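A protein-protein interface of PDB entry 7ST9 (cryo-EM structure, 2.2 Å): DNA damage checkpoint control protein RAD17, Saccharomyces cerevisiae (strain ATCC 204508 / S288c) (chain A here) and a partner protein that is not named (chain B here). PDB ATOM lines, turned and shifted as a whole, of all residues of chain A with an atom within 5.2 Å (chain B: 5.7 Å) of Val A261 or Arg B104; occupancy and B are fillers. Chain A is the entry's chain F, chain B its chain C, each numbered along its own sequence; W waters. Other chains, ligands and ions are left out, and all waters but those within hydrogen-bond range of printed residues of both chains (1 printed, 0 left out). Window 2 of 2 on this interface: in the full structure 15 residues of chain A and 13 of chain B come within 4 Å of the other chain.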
ATOM      1  N   ARG A 151      18.827  11.316 -25.581  1.00  0.00           N
ATOM      2  CA  ARG A 151      19.320  12.622 -25.152  1.00  0.00           C
ATOM      3  C   ARG A 151      19.492  13.545 -26.355  1.00  0.00           C
ATOM      4  O   ARG A 151      20.524  14.196 -26.529  1.00  0.00           O
ATOM      5  CB  ARG A 151      20.628  12.477 -24.374  1.00  0.00           C
ATOM      6  CG  ARG A 151      20.441  11.961 -22.954  1.00  0.00           C
ATOM      7  CD  ARG A 151      21.737  12.005 -22.161  1.00  0.00           C
ATOM      8  NE  ARG A 151      22.241  10.670 -21.857  1.00  0.00           N
ATOM      9  CZ  ARG A 151      21.748   9.880 -20.913  1.00  0.00           C
ATOM     10  NH1 ARG A 151      20.729  10.257 -20.156  1.00  0.00           N
ATOM     11  NH2 ARG A 151      22.291   8.681 -20.722  1.00  0.00           N
ATOM     12  N   ILE A 152      18.471  13.609 -27.208  1.00  0.00           N
ATOM     13  CA  ILE A 152      18.519  14.500 -28.363  1.00  0.00           C
ATOM     14  C   ILE A 152      18.457  15.941 -27.874  1.00  0.00           C
ATOM     15  O   ILE A 152      17.515  16.336 -27.179  1.00  0.00           O
ATOM     16  CB  ILE A 152      17.372  14.200 -29.341  1.00  0.00           C
ATOM     17  CG1 ILE A 152      17.436  12.760 -29.870  1.00  0.00           C
ATOM     18  CG2 ILE A 152      17.401  15.180 -30.510  1.00  0.00           C
ATOM     19  CD1 ILE A 152      18.816  12.142 -29.897  1.00  0.00           C
ATOM     20  N   SER A 153      19.469  16.731 -28.233  1.00  0.00           N
ATOM     21  CA  SER A 153      19.456  18.152 -27.908  1.00  0.00           C
ATOM     22  C   SER A 153      18.497  18.909 -28.815  1.00  0.00           C
ATOM     23  O   SER A 153      17.768  19.795 -28.354  1.00  0.00           O
ATOM     24  CB  SER A 153      20.865  18.731 -28.021  1.00  0.00           C
ATOM     25  OG  SER A 153      20.904  20.074 -27.574  1.00  0.00           O
ATOM     26  N   GLY A 222      17.909  18.529 -24.260  1.00  0.00           N
ATOM     27  CA  GLY A 222      18.843  17.438 -24.065  1.00  0.00           C
ATOM     28  C   GLY A 222      18.253  16.156 -23.528  1.00  0.00           C
ATOM     29  O   GLY A 222      18.998  15.324 -23.002  1.00  0.00           O
ATOM     30  N   ASP A 223      16.937  15.963 -23.638  1.00  0.00           N
ATOM     31  CA  ASP A 223      16.318  14.719 -23.200  1.00  0.00           C
ATOM     32  C   ASP A 223      15.282  14.176 -24.176  1.00  0.00           C
ATOM     33  O   ASP A 223      14.696  13.125 -23.896  1.00  0.00           O
ATOM     34  CB  ASP A 223      15.661  14.904 -21.822  1.00  0.00           C
ATOM     35  CG  ASP A 223      14.763  16.121 -21.764  1.00  0.00           C
ATOM     36  OD1 ASP A 223      13.859  16.235 -22.617  1.00  0.00           O
ATOM     37  OD2 ASP A 223      14.959  16.962 -20.862  1.00  0.00           O
ATOM     38  N   MET A 259      20.935  16.459 -33.105  1.00  0.00           N
ATOM     39  CA  MET A 259      22.110  16.629 -32.261  1.00  0.00           C
ATOM     40  C   MET A 259      21.767  16.248 -30.831  1.00  0.00           C
ATOM     41  O   MET A 259      20.711  16.641 -30.318  1.00  0.00           O
ATOM     42  CB  MET A 259      22.633  18.065 -32.307  1.00  0.00           C
ATOM     43  CG  MET A 259      24.148  18.138 -32.221  1.00  0.00           C
ATOM     44  SD  MET A 259      24.825  19.792 -32.429  1.00  0.00           S
ATOM     45  CE  MET A 259      26.417  19.567 -31.642  1.00  0.00           C
ATOM     46  N   ASP A 260      22.661  15.486 -30.198  1.00  0.00           N
ATOM     47  CA  ASP A 260      22.487  15.063 -28.816  1.00  0.00           C
ATOM     48  C   ASP A 260      23.358  15.913 -27.891  1.00  0.00           C
ATOM     49  O   ASP A 260      24.117  16.781 -28.327  1.00  0.00           O
ATOM     50  CB  ASP A 260      22.802  13.573 -28.661  1.00  0.00           C
ATOM     51  CG  ASP A 260      24.236  13.234 -29.007  1.00  0.00           C
ATOM     52  OD1 ASP A 260      25.047  14.160 -29.215  1.00  0.00           O
ATOM     53  OD2 ASP A 260      24.556  12.028 -29.066  1.00  0.00           O
ATOM     54  N   VAL A 261      23.238  15.656 -26.585  1.00  0.00           N
ATOM     55  CA  VAL A 261      23.993  16.424 -25.602  1.00  0.00           C
ATOM     56  C   VAL A 261      25.468  16.050 -25.599  1.00  0.00           C
ATOM     57  O   VAL A 261      26.305  16.857 -25.179  1.00  0.00           O
ATOM     58  CB  VAL A 261      23.399  16.236 -24.192  1.00  0.00           C
ATOM     59  CG1 VAL A 261      21.890  16.417 -24.220  1.00  0.00           C
ATOM     60  CG2 VAL A 261      23.771  14.870 -23.633  1.00  0.00           C
ATOM     61  N   HIS A 262      25.814  14.850 -26.057  1.00  0.00           N
ATOM     62  CA  HIS A 262      27.195  14.390 -26.058  1.00  0.00           C
ATOM     63  C   HIS A 262      28.013  14.972 -27.205  1.00  0.00           C
ATOM     64  O   HIS A 262      29.131  14.504 -27.445  1.00  0.00           O
ATOM     65  CB  HIS A 262      27.239  12.861 -26.120  1.00  0.00           C
ATOM     66  CG  HIS A 262      26.442  12.191 -25.045  1.00  0.00           C
ATOM     67  ND1 HIS A 262      26.597  12.487 -23.708  1.00  0.00           N
ATOM     68  CD2 HIS A 262      25.484  11.237 -25.110  1.00  0.00           C
ATOM     69  CE1 HIS A 262      25.769  11.745 -22.996  1.00  0.00           C
ATOM     70  NE2 HIS A 262      25.081  10.978 -23.822  1.00  0.00           N
ATOM     71  N   GLY A 263      27.494  15.973 -27.910  1.00  0.00           N
ATOM     72  CA  GLY A 263      28.223  16.567 -29.010  1.00  0.00           C
ATOM     73  C   GLY A 263      28.231  15.750 -30.279  1.00  0.00           C
ATOM     74  O   GLY A 263      29.141  15.910 -31.098  1.00  0.00           O
ATOM     75  N   LEU A 311      31.284  14.155 -34.759  1.00  0.00           N
ATOM     76  CA  LEU A 311      31.551  14.651 -33.418  1.00  0.00           C
ATOM     77  C   LEU A 311      31.785  16.155 -33.445  1.00  0.00           C
ATOM     78  O   LEU A 311      32.297  16.708 -34.421  1.00  0.00           O
ATOM     79  CB  LEU A 311      32.769  13.949 -32.811  1.00  0.00           C
ATOM     80  CG  LEU A 311      32.527  12.547 -32.249  1.00  0.00           C
ATOM     81  CD1 LEU A 311      33.847  11.831 -32.023  1.00  0.00           C
ATOM     82  CD2 LEU A 311      31.727  12.615 -30.958  1.00  0.00           C
ATOM     83  N   GLU A 312      31.404  16.812 -32.355  1.00  0.00           N
ATOM     84  CA  GLU A 312      31.581  18.245 -32.192  1.00  0.00           C
ATOM     85  C   GLU A 312      32.970  18.545 -31.632  1.00  0.00           C
ATOM     86  O   GLU A 312      33.607  17.700 -30.999  1.00  0.00           O
ATOM     87  CB  GLU A 312      30.490  18.804 -31.271  1.00  0.00           C
ATOM     88  CG  GLU A 312      30.762  20.185 -30.696  1.00  0.00           C
ATOM     89  CD  GLU A 312      29.543  20.792 -30.030  1.00  0.00           C
ATOM     90  OE1 GLU A 312      28.571  20.051 -29.775  1.00  0.00           O
ATOM     91  OE2 GLU A 312      29.555  22.012 -29.763  1.00  0.00           O
ATOM     92  N   LYS A 313      33.440  19.765 -31.881  1.00  0.00           N
ATOM     93  CA  LYS A 313      34.739  20.179 -31.374  1.00  0.00           C
ATOM     94  C   LYS A 313      34.714  20.272 -29.851  1.00  0.00           C
ATOM     95  O   LYS A 313      33.657  20.310 -29.217  1.00  0.00           O
ATOM     96  CB  LYS A 313      35.151  21.523 -31.975  1.00  0.00           C
ATOM     97  CG  LYS A 313      35.193  21.552 -33.496  1.00  0.00           C
ATOM     98  CD  LYS A 313      36.354  20.733 -34.047  1.00  0.00           C
ATOM     99  CE  LYS A 313      37.621  21.563 -34.163  1.00  0.00           C
ATOM    100  NZ  LYS A 313      38.699  20.839 -34.889  1.00  0.00           N
ATOM    101  N   GLU A 314      35.912  20.313 -29.261  1.00  0.00           N
ATOM    102  CA  GLU A 314      36.020  20.258 -27.806  1.00  0.00           C
ATOM    103  C   GLU A 314      35.306  21.433 -27.146  1.00  0.00           C
ATOM    104  O   GLU A 314      34.575  21.250 -26.166  1.00  0.00           O
ATOM    105  CB  GLU A 314      37.492  20.228 -27.387  1.00  0.00           C
ATOM    106  CG  GLU A 314      38.345  21.346 -27.988  1.00  0.00           C
ATOM    107  CD  GLU A 314      38.901  22.309 -26.949  1.00  0.00           C
ATOM    108  OE1 GLU A 314      38.812  22.016 -25.737  1.00  0.00           O
ATOM    109  OE2 GLU A 314      39.436  23.365 -27.347  1.00  0.00           O
ATOM    110  N   SER B 102      41.216  17.382 -30.872  1.00  0.00           N
ATOM    111  CA  SER B 102      40.380  18.562 -30.702  1.00  0.00           C
ATOM    112  C   SER B 102      38.889  18.247 -30.759  1.00  0.00           C
ATOM    113  O   SER B 102      38.074  19.174 -30.797  1.00  0.00           O
ATOM    114  CB  SER B 102      40.730  19.606 -31.764  1.00  0.00           C
ATOM    115  OG  SER B 102      40.382  19.152 -33.060  1.00  0.00           O
ATOM    116  N   THR B 103      38.514  16.972 -30.764  1.00  0.00           N
ATOM    117  CA  THR B 103      37.119  16.563 -30.816  1.00  0.00           C
ATOM    118  C   THR B 103      36.697  15.969 -29.478  1.00  0.00           C
ATOM    119  O   THR B 103      37.520  15.472 -28.704  1.00  0.00           O
ATOM    120  CB  THR B 103      36.880  15.542 -31.937  1.00  0.00           C
ATOM    121  OG1 THR B 103      37.959  14.601 -31.978  1.00  0.00           O
ATOM    122  CG2 THR B 103      36.762  16.242 -33.284  1.00  0.00           C
ATOM    123  N   ARG B 104      35.395  16.029 -29.214  1.00  0.00           N
ATOM    124  CA  ARG B 104      34.863  15.551 -27.950  1.00  0.00           C
ATOM    125  C   ARG B 104      34.889  14.025 -27.889  1.00  0.00           C
ATOM    126  O   ARG B 104      35.020  13.333 -28.902  1.00  0.00           O
ATOM    127  CB  ARG B 104      33.434  16.053 -27.744  1.00  0.00           C
ATOM    128  CG  ARG B 104      33.321  17.571 -27.674  1.00  0.00           C
ATOM    129  CD  ARG B 104      31.908  18.053 -27.348  1.00  0.00           C
ATOM    130  NE  ARG B 104      31.212  17.208 -26.383  1.00  0.00           N
ATOM    131  CZ  ARG B 104      30.054  17.522 -25.817  1.00  0.00           C
ATOM    132  NH1 ARG B 104      29.433  18.656 -26.097  1.00  0.00           N
ATOM    133  NH2 ARG B 104      29.506  16.677 -24.948  1.00  0.00           N
ATOM    134  N   GLN B 105      34.762  13.507 -26.671  1.00  0.00           N
ATOM    135  CA  GLN B 105      34.743  12.069 -26.453  1.00  0.00           C
ATOM    136  C   GLN B 105      33.474  11.454 -27.036  1.00  0.00           C
ATOM    137  O   GLN B 105      32.465  12.129 -27.256  1.00  0.00           O
ATOM    138  CB  GLN B 105      34.840  11.754 -24.960  1.00  0.00           C
ATOM    139  CG  GLN B 105      36.199  11.244 -24.510  1.00  0.00           C
ATOM    140  CD  GLN B 105      36.503   9.846 -25.017  1.00  0.00           C
ATOM    141  OE1 GLN B 105      36.102   9.467 -26.116  1.00  0.00           O
ATOM    142  NE2 GLN B 105      37.211   9.067 -24.206  1.00  0.00           N
ATOM    143  N   ILE B 106      33.536  10.144 -27.283  1.00  0.00           N
ATOM    144  CA  ILE B 106      32.414   9.448 -27.908  1.00  0.00           C
ATOM    145  C   ILE B 106      31.171   9.550 -27.031  1.00  0.00           C
ATOM    146  O   ILE B 106      30.073   9.856 -27.511  1.00  0.00           O
ATOM    147  CB  ILE B 106      32.782   7.980 -28.191  1.00  0.00           C
ATOM    148  CG1 ILE B 106      33.987   7.898 -29.135  1.00  0.00           C
ATOM    149  CG2 ILE B 106      31.590   7.238 -28.778  1.00  0.00           C
ATOM    150  CD1 ILE B 106      33.655   8.167 -30.586  1.00  0.00           C
ATOM    151  N   SER B 108      31.478  11.155 -23.722  1.00  0.00           N
ATOM    152  CA  SER B 108      31.992  11.952 -22.609  1.00  0.00           C
ATOM    153  C   SER B 108      32.701  11.069 -21.586  1.00  0.00           C
ATOM    154  O   SER B 108      32.540  11.235 -20.375  1.00  0.00           O
ATOM    155  CB  SER B 108      30.871  12.756 -21.948  1.00  0.00           C
ATOM    156  OG  SER B 108      31.390  13.666 -20.994  1.00  0.00           O
ATOM    157  N   LYS B 112      40.463  11.689 -23.944  1.00  0.00           N
ATOM    158  CA  LYS B 112      40.901  10.794 -25.004  1.00  0.00           C
ATOM    159  C   LYS B 112      42.388  10.491 -24.854  1.00  0.00           C
ATOM    160  O   LYS B 112      43.135  11.221 -24.199  1.00  0.00           O
ATOM    161  CB  LYS B 112      40.622  11.411 -26.376  1.00  0.00           C
ATOM    162  CG  LYS B 112      39.237  12.029 -26.510  1.00  0.00           C
ATOM    163  CD  LYS B 112      39.075  12.759 -27.832  1.00  0.00           C
ATOM    164  CE  LYS B 112      38.558  11.832 -28.918  1.00  0.00           C
ATOM    165  NZ  LYS B 112      38.341  12.543 -30.207  1.00  0.00           N
ATOM    166  N   ASN B 140      41.405  17.791 -22.854  1.00  0.00           N
ATOM    167  CA  ASN B 140      40.586  16.780 -23.509  1.00  0.00           C
ATOM    168  C   ASN B 140      41.372  15.543 -23.925  1.00  0.00           C
ATOM    169  O   ASN B 140      40.761  14.498 -24.175  1.00  0.00           O
ATOM    170  CB  ASN B 140      39.903  17.383 -24.742  1.00  0.00           C
ATOM    171  CG  ASN B 140      38.979  16.403 -25.439  1.00  0.00           C
ATOM    172  OD1 ASN B 140      38.008  15.925 -24.855  1.00  0.00           O
ATOM    173  ND2 ASN B 140      39.276  16.101 -26.699  1.00  0.00           N
HETATM  174  O   HOH W   1      41.754  22.094 -34.358  1.00  0.00           O
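Among the printed residues, pairs that only touch across the chains: Gly A263 with Arg B104 (3.6 Å), Leu A311 with Arg B104 (3.7 Å), Leu A311 with Gln B105 (3.8 Å), Leu A311 with Ile B106 (3.9 Å), Glu A312 with Thr B103 (3.7 Å), Lys A313 with Arg B104 (3.2 Å) and Glu A314 with Arg B104 (3.8 Å).
Water W1 bridges the side-chain amino group (NZ) of Lys A313 (3.3 Å) and the side-chain hydroxyl (OG) of Ser B102 (3.5 Å).
Of the printed residues of chain B, His A262 touches Arg B104 (3.2 Å).
Printed residues of chain B within 4 Å of Leu A311: Arg B104, Gln B105 and Ile B106.
Printed residues of chain B within 4 Å of Glu A312: Thr B103 and Arg B104.
Of the printed residues of chain B, Lys A313 touches Ser B102 (3.0 Å) and Arg B104 (3.2 Å).
Of the printed residues of chain A, Thr B103 touches Glu A312.
Arg B104 touches just these residues of chain A: Val A261, His A262, Gly A263, Leu A311, Glu A312, Lys A313 and Glu A314.
The nearest printed residue of chain A that does not touch Arg B104 is Asp A260 (6.1 Å).
Of the 8 printed residues of chain B, 5 touch a printed residue of chain A.
Printed residues of chain B that touch a printed residue of chain A: Ser B102, Thr B103, Arg B104, Gln B105 and Ile B106.
Along chain B the printed residues that touch a printed residue of chain A span positions 102 to 106.
Hydrophobic or aromatic side chains of chain A within 4 Å of the printed part of chain B: Leu A311.
Among the printed residues, no Asp or Glu carboxylate lies within 4 Å of a Lys or Arg side-chain nitrogen of the other chain.
The side-chain carboxylate (OD1) of Asp A260 lies close to the backbone NH (N) of His A262, 3.3 Å away.
OG1 of Thr B103 sits at hydrogen-bond distance from NZ of Lys B112 (2.7 Å).
The guanidinium group (NE) of Arg A151 lies within hydrogen-bond range of a ring nitrogen (NE2) of His A262, at 3.5 Å.
O of Gly A263 sits at hydrogen-bond distance from N of Glu A312.
The backbone carbonyl oxygen (O) of Thr B103 sits at hydrogen-bond distance from the side-chain amide nitrogen (ND2) of Asn B140, 2.7 Å away.
The backbone carbonyl oxygen (O) of Arg A151 sits at hydrogen-bond distance from the backbone NH (N) of Val A261.
The side-chain hydroxyl (OG) of Ser B102 lies within hydrogen-bond range of the side-chain amino group (NZ) of Lys A313 (3.0 Å).
The backbone carbonyl oxygen (O) of Ser B102 lies within hydrogen-bond range of the backbone NH (N) of Glu A314, at 2.9 Å.
The backbone carbonyl oxygen (O) of Glu A312 lies within hydrogen-bond range of the backbone NH (N) of Arg B104.
The backbone carbonyl oxygen (O) of His A262 lies close to the guanidinium group (NH2) of Arg B104.
O of Val A261 lies within hydrogen-bond range of NH2 of Arg B104, at 3.2 Å.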
